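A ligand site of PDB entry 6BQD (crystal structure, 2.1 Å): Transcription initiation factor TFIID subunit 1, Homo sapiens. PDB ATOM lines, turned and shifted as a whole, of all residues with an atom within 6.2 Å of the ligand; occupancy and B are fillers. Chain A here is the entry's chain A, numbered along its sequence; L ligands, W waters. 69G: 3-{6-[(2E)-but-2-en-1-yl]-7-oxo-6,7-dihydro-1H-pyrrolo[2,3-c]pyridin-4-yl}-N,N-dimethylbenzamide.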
ATOM      1  N   TRP A  26       7.830 -23.122  19.878  1.00  0.00           N
ATOM      2  CA  TRP A  26       6.874 -22.448  18.994  1.00  0.00           C
ATOM      3  C   TRP A  26       7.263 -20.982  18.702  1.00  0.00           C
ATOM      4  O   TRP A  26       7.016 -20.521  17.598  1.00  0.00           O
ATOM      5  CB  TRP A  26       5.419 -22.536  19.532  1.00  0.00           C
ATOM      6  CG  TRP A  26       5.199 -21.880  20.878  1.00  0.00           C
ATOM      7  CD1 TRP A  26       5.178 -22.503  22.102  1.00  0.00           C
ATOM      8  CD2 TRP A  26       4.984 -20.474  21.143  1.00  0.00           C
ATOM      9  NE1 TRP A  26       4.974 -21.566  23.111  1.00  0.00           N
ATOM     10  CE2 TRP A  26       4.848 -20.317  22.543  1.00  0.00           C
ATOM     11  CE3 TRP A  26       4.892 -19.347  20.335  1.00  0.00           C
ATOM     12  CZ2 TRP A  26       4.643 -19.077  23.135  1.00  0.00           C
ATOM     13  CZ3 TRP A  26       4.685 -18.104  20.937  1.00  0.00           C
ATOM     14  CH2 TRP A  26       4.566 -17.980  22.310  1.00  0.00           C
ATOM     15  N   PRO A  27       7.894 -20.236  19.621  1.00  0.00           N
ATOM     16  CA  PRO A  27       8.243 -18.839  19.294  1.00  0.00           C
ATOM     17  C   PRO A  27       9.201 -18.699  18.138  1.00  0.00           C
ATOM     18  O   PRO A  27       9.313 -17.591  17.604  1.00  0.00           O
ATOM     19  CB  PRO A  27       8.878 -18.325  20.590  1.00  0.00           C
ATOM     20  CG  PRO A  27       8.356 -19.206  21.647  1.00  0.00           C
ATOM     21  CD  PRO A  27       8.295 -20.566  20.991  1.00  0.00           C
ATOM     22  N   PHE A  28       9.919 -19.767  17.740  1.00  0.00           N
ATOM     23  CA  PHE A  28      10.934 -19.734  16.697  1.00  0.00           C
ATOM     24  C   PHE A  28      10.469 -20.379  15.405  1.00  0.00           C
ATOM     25  O   PHE A  28      11.236 -20.451  14.463  1.00  0.00           O
ATOM     26  CB  PHE A  28      12.245 -20.433  17.171  1.00  0.00           C
ATOM     27  CG  PHE A  28      12.792 -19.829  18.421  1.00  0.00           C
ATOM     28  CD1 PHE A  28      13.565 -18.693  18.364  1.00  0.00           C
ATOM     29  CD2 PHE A  28      12.476 -20.364  19.664  1.00  0.00           C
ATOM     30  CE1 PHE A  28      14.038 -18.094  19.521  1.00  0.00           C
ATOM     31  CE2 PHE A  28      12.945 -19.776  20.848  1.00  0.00           C
ATOM     32  CZ  PHE A  28      13.739 -18.661  20.793  1.00  0.00           C
ATOM     33  N   HIS A  29       9.205 -20.831  15.341  1.00  0.00           N
ATOM     34  CA  HIS A  29       8.723 -21.528  14.157  1.00  0.00           C
ATOM     35  C   HIS A  29       8.506 -20.571  12.994  1.00  0.00           C
ATOM     36  O   HIS A  29       8.713 -20.962  11.841  1.00  0.00           O
ATOM     37  CB  HIS A  29       7.435 -22.283  14.481  1.00  0.00           C
ATOM     38  CG  HIS A  29       7.670 -23.488  15.366  1.00  0.00           C
ATOM     39  ND1 HIS A  29       6.704 -24.450  15.572  1.00  0.00           N
ATOM     40  CD2 HIS A  29       8.751 -23.873  16.088  1.00  0.00           C
ATOM     41  CE1 HIS A  29       7.194 -25.392  16.368  1.00  0.00           C
ATOM     42  NE2 HIS A  29       8.426 -25.056  16.696  1.00  0.00           N
ATOM     43  N   HIS A  30       8.117 -19.323  13.265  1.00  0.00           N
ATOM     44  CA  HIS A  30       7.638 -18.395  12.256  1.00  0.00           C
ATOM     45  C   HIS A  30       8.223 -17.016  12.510  1.00  0.00           C
ATOM     46  O   HIS A  30       8.564 -16.692  13.655  1.00  0.00           O
ATOM     47  CB  HIS A  30       6.111 -18.323  12.267  1.00  0.00           C
ATOM     48  CG  HIS A  30       5.448 -19.668  12.192  1.00  0.00           C
ATOM     49  ND1 HIS A  30       5.352 -20.386  11.024  1.00  0.00           N
ATOM     50  CD2 HIS A  30       4.896 -20.448  13.155  1.00  0.00           C
ATOM     51  CE1 HIS A  30       4.750 -21.537  11.258  1.00  0.00           C
ATOM     52  NE2 HIS A  30       4.455 -21.597  12.548  1.00  0.00           N
ATOM     53  N   PRO A  31       8.314 -16.160  11.479  1.00  0.00           N
ATOM     54  CA  PRO A  31       8.755 -14.777  11.688  1.00  0.00           C
ATOM     55  C   PRO A  31       7.931 -14.093  12.768  1.00  0.00           C
ATOM     56  O   PRO A  31       6.757 -14.406  12.986  1.00  0.00           O
ATOM     57  CB  PRO A  31       8.536 -14.132  10.324  1.00  0.00           C
ATOM     58  CG  PRO A  31       8.312 -15.293   9.338  1.00  0.00           C
ATOM     59  CD  PRO A  31       7.740 -16.379  10.138  1.00  0.00           C
ATOM     60  N   VAL A  32       8.551 -13.156  13.471  1.00  0.00           N
ATOM     61  CA  VAL A  32       7.838 -12.433  14.493  1.00  0.00           C
ATOM     62  C   VAL A  32       6.755 -11.575  13.835  1.00  0.00           C
ATOM     63  O   VAL A  32       6.970 -10.973  12.774  1.00  0.00           O
ATOM     64  CB  VAL A  32       8.797 -11.561  15.309  1.00  0.00           C
ATOM     65  CG1 VAL A  32       8.006 -10.579  16.171  1.00  0.00           C
ATOM     66  CG2 VAL A  32       9.695 -12.450  16.194  1.00  0.00           C
ATOM     67  N   ASN A  33       5.593 -11.528  14.446  1.00  0.00           N
ATOM     68  CA  ASN A  33       4.570 -10.561  14.077  1.00  0.00           C
ATOM     69  C   ASN A  33       4.735  -9.347  14.984  1.00  0.00           C
ATOM     70  O   ASN A  33       4.677  -9.453  16.224  1.00  0.00           O
ATOM     71  CB  ASN A  33       3.173 -11.181  14.177  1.00  0.00           C
ATOM     72  CG  ASN A  33       2.076 -10.267  13.680  1.00  0.00           C
ATOM     73  OD1 ASN A  33       2.164  -9.041  13.812  1.00  0.00           O
ATOM     74  ND2 ASN A  33       1.032 -10.844  13.097  1.00  0.00           N
ATOM     75  N   LYS A  34       4.998  -8.192  14.386  1.00  0.00           N
ATOM     76  CA  LYS A  34       5.228  -6.988  15.167  1.00  0.00           C
ATOM     77  C   LYS A  34       4.048  -6.664  16.100  1.00  0.00           C
ATOM     78  O   LYS A  34       4.243  -6.077  17.168  1.00  0.00           O
ATOM     79  CB  LYS A  34       5.536  -5.853  14.188  1.00  0.00           C
ATOM     80  CG  LYS A  34       5.666  -4.482  14.743  1.00  0.00           C
ATOM     81  CD  LYS A  34       5.644  -3.510  13.572  1.00  0.00           C
ATOM     82  CE  LYS A  34       5.840  -2.065  14.022  1.00  0.00           C
ATOM     83  NZ  LYS A  34       5.691  -1.160  12.841  1.00  0.00           N
ATOM     84  N   PHE A  36       2.655  -8.691  18.038  1.00  0.00           N
ATOM     85  CA  PHE A  36       2.857  -9.438  19.264  1.00  0.00           C
ATOM     86  C   PHE A  36       4.119  -9.023  19.986  1.00  0.00           C
ATOM     87  O   PHE A  36       4.177  -9.147  21.215  1.00  0.00           O
ATOM     88  CB  PHE A  36       2.890 -10.950  18.971  1.00  0.00           C
ATOM     89  CG  PHE A  36       1.711 -11.448  18.158  1.00  0.00           C
ATOM     90  CD1 PHE A  36       0.444 -10.883  18.293  1.00  0.00           C
ATOM     91  CD2 PHE A  36       1.885 -12.469  17.232  1.00  0.00           C
ATOM     92  CE1 PHE A  36      -0.619 -11.340  17.555  1.00  0.00           C
ATOM     93  CE2 PHE A  36       0.828 -12.947  16.471  1.00  0.00           C
ATOM     94  CZ  PHE A  36      -0.422 -12.377  16.619  1.00  0.00           C
ATOM     95  N   VAL A  37       5.125  -8.550  19.264  1.00  0.00           N
ATOM     96  CA  VAL A  37       6.408  -8.128  19.822  1.00  0.00           C
ATOM     97  C   VAL A  37       6.767  -6.781  19.197  1.00  0.00           C
ATOM     98  O   VAL A  37       7.524  -6.739  18.215  1.00  0.00           O
ATOM     99  CB  VAL A  37       7.502  -9.177  19.588  1.00  0.00           C
ATOM    100  CG1 VAL A  37       8.719  -8.857  20.418  1.00  0.00           C
ATOM    101  CG2 VAL A  37       6.999 -10.581  19.973  1.00  0.00           C
ATOM    102  N   TYR A  40      10.442  -5.787  18.054  1.00  0.00           N
ATOM    103  CA  TYR A  40      11.372  -6.818  17.599  1.00  0.00           C
ATOM    104  C   TYR A  40      12.254  -6.317  16.450  1.00  0.00           C
ATOM    105  O   TYR A  40      13.484  -6.419  16.509  1.00  0.00           O
ATOM    106  CB  TYR A  40      10.637  -8.077  17.184  1.00  0.00           C
ATOM    107  CG  TYR A  40      11.609  -9.211  17.026  1.00  0.00           C
ATOM    108  CD1 TYR A  40      12.166  -9.799  18.151  1.00  0.00           C
ATOM    109  CD2 TYR A  40      12.005  -9.684  15.762  1.00  0.00           C
ATOM    110  CE1 TYR A  40      13.078 -10.829  18.057  1.00  0.00           C
ATOM    111  CE2 TYR A  40      12.933 -10.743  15.651  1.00  0.00           C
ATOM    112  CZ  TYR A  40      13.450 -11.313  16.816  1.00  0.00           C
ATOM    113  OH  TYR A  40      14.368 -12.334  16.796  1.00  0.00           O
ATOM    114  N   PRO A  47      16.507 -10.721  11.064  1.00  0.00           N
ATOM    115  CA  PRO A  47      15.612 -11.717  11.655  1.00  0.00           C
ATOM    116  C   PRO A  47      15.797 -13.080  10.999  1.00  0.00           C
ATOM    117  O   PRO A  47      16.220 -13.184   9.840  1.00  0.00           O
ATOM    118  CB  PRO A  47      14.216 -11.153  11.397  1.00  0.00           C
ATOM    119  CG  PRO A  47      14.427  -9.708  10.919  1.00  0.00           C
ATOM    120  CD  PRO A  47      15.790  -9.647  10.340  1.00  0.00           C
ATOM    121  N   MET A  48      15.466 -14.137  11.752  1.00  0.00           N
ATOM    122  CA  MET A  48      15.560 -15.498  11.252  1.00  0.00           C
ATOM    123  C   MET A  48      14.615 -16.390  12.065  1.00  0.00           C
ATOM    124  O   MET A  48      14.410 -16.173  13.269  1.00  0.00           O
ATOM    125  CB  MET A  48      16.988 -16.050  11.335  1.00  0.00           C
ATOM    126  CG  MET A  48      17.185 -17.436  10.625  1.00  0.00           C
ATOM    127  SD  MET A  48      16.580 -17.488   8.907  1.00  0.00           S
ATOM    128  CE  MET A  48      17.362 -16.043   8.167  1.00  0.00           C
ATOM    129  N   ASP A  49      14.055 -17.392  11.392  1.00  0.00           N
ATOM    130  CA  ASP A  49      13.123 -18.308  12.041  1.00  0.00           C
ATOM    131  C   ASP A  49      13.121 -19.627  11.281  1.00  0.00           C
ATOM    132  O   ASP A  49      13.598 -19.687  10.148  1.00  0.00           O
ATOM    133  CB  ASP A  49      11.732 -17.693  12.061  1.00  0.00           C
ATOM    134  CG  ASP A  49      11.171 -17.569  10.633  1.00  0.00           C
ATOM    135  OD1 ASP A  49      10.739 -18.619  10.108  1.00  0.00           O
ATOM    136  OD2 ASP A  49      11.193 -16.455  10.032  1.00  0.00           O
ATOM    137  N   ILE A  75      19.529 -17.534  14.707  1.00  0.00           N
ATOM    138  CA  ILE A  75      18.380 -17.556  15.594  1.00  0.00           C
ATOM    139  C   ILE A  75      18.836 -17.397  17.045  1.00  0.00           C
ATOM    140  O   ILE A  75      18.239 -16.619  17.815  1.00  0.00           O
ATOM    141  CB  ILE A  75      17.540 -18.845  15.413  1.00  0.00           C
ATOM    142  CG1 ILE A  75      16.960 -18.921  13.999  1.00  0.00           C
ATOM    143  CG2 ILE A  75      16.431 -18.892  16.474  1.00  0.00           C
ATOM    144  CD1 ILE A  75      16.439 -20.240  13.657  1.00  0.00           C
ATOM    145  N   ASN A  78      20.160 -13.700  17.653  1.00  0.00           N
ATOM    146  CA  ASN A  78      19.084 -12.732  17.826  1.00  0.00           C
ATOM    147  C   ASN A  78      18.422 -12.883  19.196  1.00  0.00           C
ATOM    148  O   ASN A  78      18.053 -11.887  19.823  1.00  0.00           O
ATOM    149  CB  ASN A  78      18.071 -12.897  16.675  1.00  0.00           C
ATOM    150  CG  ASN A  78      18.669 -12.446  15.319  1.00  0.00           C
ATOM    151  OD1 ASN A  78      19.645 -11.710  15.299  1.00  0.00           O
ATOM    152  ND2 ASN A  78      18.078 -12.908  14.199  1.00  0.00           N
ATOM    153  N   SER A  79      18.306 -14.115  19.693  1.00  0.00           N
ATOM    154  CA  SER A  79      17.662 -14.310  20.986  1.00  0.00           C
ATOM    155  C   SER A  79      18.518 -13.785  22.137  1.00  0.00           C
ATOM    156  O   SER A  79      17.993 -13.140  23.056  1.00  0.00           O
ATOM    157  CB  SER A  79      17.299 -15.779  21.197  1.00  0.00           C
ATOM    158  OG  SER A  79      16.585 -15.938  22.415  1.00  0.00           O
ATOM    159  N   TYR A  82      18.007  -9.989  21.856  1.00  0.00           N
ATOM    160  CA  TYR A  82      16.709  -9.412  22.201  1.00  0.00           C
ATOM    161  C   TYR A  82      16.276  -9.773  23.622  1.00  0.00           C
ATOM    162  O   TYR A  82      15.680  -8.941  24.313  1.00  0.00           O
ATOM    163  CB  TYR A  82      15.644  -9.868  21.207  1.00  0.00           C
ATOM    164  CG  TYR A  82      14.335  -9.130  21.393  1.00  0.00           C
ATOM    165  CD1 TYR A  82      14.211  -7.805  21.003  1.00  0.00           C
ATOM    166  CD2 TYR A  82      13.241  -9.741  21.988  1.00  0.00           C
ATOM    167  CE1 TYR A  82      13.036  -7.088  21.194  1.00  0.00           C
ATOM    168  CE2 TYR A  82      12.036  -9.017  22.169  1.00  0.00           C
ATOM    169  CZ  TYR A  82      11.963  -7.693  21.780  1.00  0.00           C
ATOM    170  OH  TYR A  82      10.813  -6.959  21.936  1.00  0.00           O
ATOM    171  N   ASN A  83      16.563 -10.994  24.082  1.00  0.00           N
ATOM    172  CA  ASN A  83      16.026 -11.476  25.342  1.00  0.00           C
ATOM    173  C   ASN A  83      17.049 -11.626  26.440  1.00  0.00           C
ATOM    174  O   ASN A  83      16.647 -11.714  27.608  1.00  0.00           O
ATOM    175  CB  ASN A  83      15.366 -12.855  25.161  1.00  0.00           C
ATOM    176  CG  ASN A  83      14.332 -12.865  24.118  1.00  0.00           C
ATOM    177  OD1 ASN A  83      13.303 -12.197  24.251  1.00  0.00           O
ATOM    178  ND2 ASN A  83      14.542 -13.680  23.091  1.00  0.00           N
ATOM    179  N   TYR A  89      13.741 -17.995  26.397  1.00  0.00           N
ATOM    180  CA  TYR A  89      13.783 -18.061  24.927  1.00  0.00           C
ATOM    181  C   TYR A  89      15.166 -18.477  24.454  1.00  0.00           C
ATOM    182  O   TYR A  89      15.302 -19.228  23.473  1.00  0.00           O
ATOM    183  CB  TYR A  89      13.447 -16.704  24.299  1.00  0.00           C
ATOM    184  CG  TYR A  89      12.027 -16.232  24.518  1.00  0.00           C
ATOM    185  CD1 TYR A  89      10.967 -16.779  23.797  1.00  0.00           C
ATOM    186  CD2 TYR A  89      11.746 -15.227  25.426  1.00  0.00           C
ATOM    187  CE1 TYR A  89       9.674 -16.356  24.008  1.00  0.00           C
ATOM    188  CE2 TYR A  89      10.451 -14.781  25.639  1.00  0.00           C
ATOM    189  CZ  TYR A  89       9.424 -15.353  24.913  1.00  0.00           C
ATOM    190  OH  TYR A  89       8.147 -14.940  25.100  1.00  0.00           O
HETATM  191  C4  69G L   1      11.946 -15.502  18.849  1.00  0.00           C
HETATM  192  C14 69G L   1      11.591 -14.014  20.722  1.00  0.00           C
HETATM  193  C6  69G L   1       9.681 -14.855  19.583  1.00  0.00           C
HETATM  194  C7  69G L   1       8.823 -14.204  20.426  1.00  0.00           C
HETATM  195  C8  69G L   1       9.388 -13.387  21.512  1.00  0.00           C
HETATM  196  C9  69G L   1       8.868 -12.580  22.562  1.00  0.00           C
HETATM  197  C10 69G L   1       9.900 -12.056  23.276  1.00  0.00           C
HETATM  198  C13 69G L   1      10.788 -13.305  21.630  1.00  0.00           C
HETATM  199  C3  69G L   1      12.005 -14.913  17.492  1.00  0.00           C
HETATM  200  C1  69G L   1      11.747 -15.128  15.088  1.00  0.00           C
HETATM  201  C2  69G L   1      11.708 -15.687  16.492  1.00  0.00           C
HETATM  202  N5  69G L   1      11.035 -14.750  19.726  1.00  0.00           N
HETATM  203  N11 69G L   1      11.066 -12.501  22.724  1.00  0.00           N
HETATM  204  O15 69G L   1      12.803 -13.949  20.817  1.00  0.00           O
HETATM  205  C16 69G L   1       7.335 -14.303  20.240  1.00  0.00           C
HETATM  206  C17 69G L   1       6.437 -14.366  21.322  1.00  0.00           C
HETATM  207  C18 69G L   1       5.067 -14.440  21.096  1.00  0.00           C
HETATM  208  C19 69G L   1       4.582 -14.407  19.789  1.00  0.00           C
HETATM  209  C20 69G L   1       5.462 -14.350  18.695  1.00  0.00           C
HETATM  210  C21 69G L   1       6.841 -14.284  18.927  1.00  0.00           C
HETATM  211  C22 69G L   1       4.985 -14.306  17.286  1.00  0.00           C
HETATM  212  O23 69G L   1       5.136 -13.273  16.626  1.00  0.00           O
HETATM  213  N24 69G L   1       4.393 -15.332  16.682  1.00  0.00           N
HETATM  214  C25 69G L   1       3.998 -15.148  15.276  1.00  0.00           C
HETATM  215  C26 69G L   1       4.187 -16.596  17.384  1.00  0.00           C
HETATM  216  O   HOH W   1      14.977 -13.464  19.006  1.00  0.00           O
HETATM  217  O   HOH W   2       7.541 -15.878  15.989  1.00  0.00           O
HETATM  218  O   HOH W   3       7.846 -12.130  25.759  1.00  0.00           O
HETATM  219  O   HOH W   4       6.578 -18.451  15.771  1.00  0.00           O
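ND2 of Asn 83 is in hydrogen-bond range of OG of Ser 79.
CZ3 of Trp 26 touches C18 of the ligand (3.7 Å). Pro 27 touches the ligand (O to C2, 3.3 Å). CE1 of Phe 28 touches C4 of the ligand, at 3.4 Å. O of His 30 touches C1 of the ligand, 3.8 Å away. Pro 31 touches the ligand (O to C25, 3.7 Å). Val 32 touches the ligand (CA to O23, 3.5 Å). CD2 of Phe 36 touches O23 of the ligand, at 3.4 Å. Val 37 touches the ligand (CG2 to C16, 3.7 Å). Tyr 40 touches the ligand (OH to C3, 3.6 Å). Met 48 touches the ligand. Asp 49 touches the ligand. Tyr 82 touches the ligand. Tyr 89 touches the ligand. Hydrophobic or aromatic side chains within 4 Å of the ligand: Trp 26, Pro 27, Phe 28, Val 32, Phe 36, Val 37, Tyr 40, Tyr 82 and Tyr 89. 15 residues have an atom within 4 Å of the ligand: Trp 26, Pro 27, Phe 28, His 30, Pro 31, Val 32, Asn 33, Phe 36, Val 37, Tyr 40, Met 48, Asp 49, Tyr 82, Asn 83 and Tyr 89.
Water W1 lies within hydrogen-bond range of the side-chain hydroxyl of Tyr 40 (2.6 Å), an oxygen (O15) of the ligand (2.9 Å) and the backbone NH of Ser 79 (3.5 Å).
N11 of the ligand lies within hydrogen-bond range of OD1 of Asn 83 (2.7 Å). N of Asn 33 sits at hydrogen-bond distance from O23 of the ligand, 2.8 Å away.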
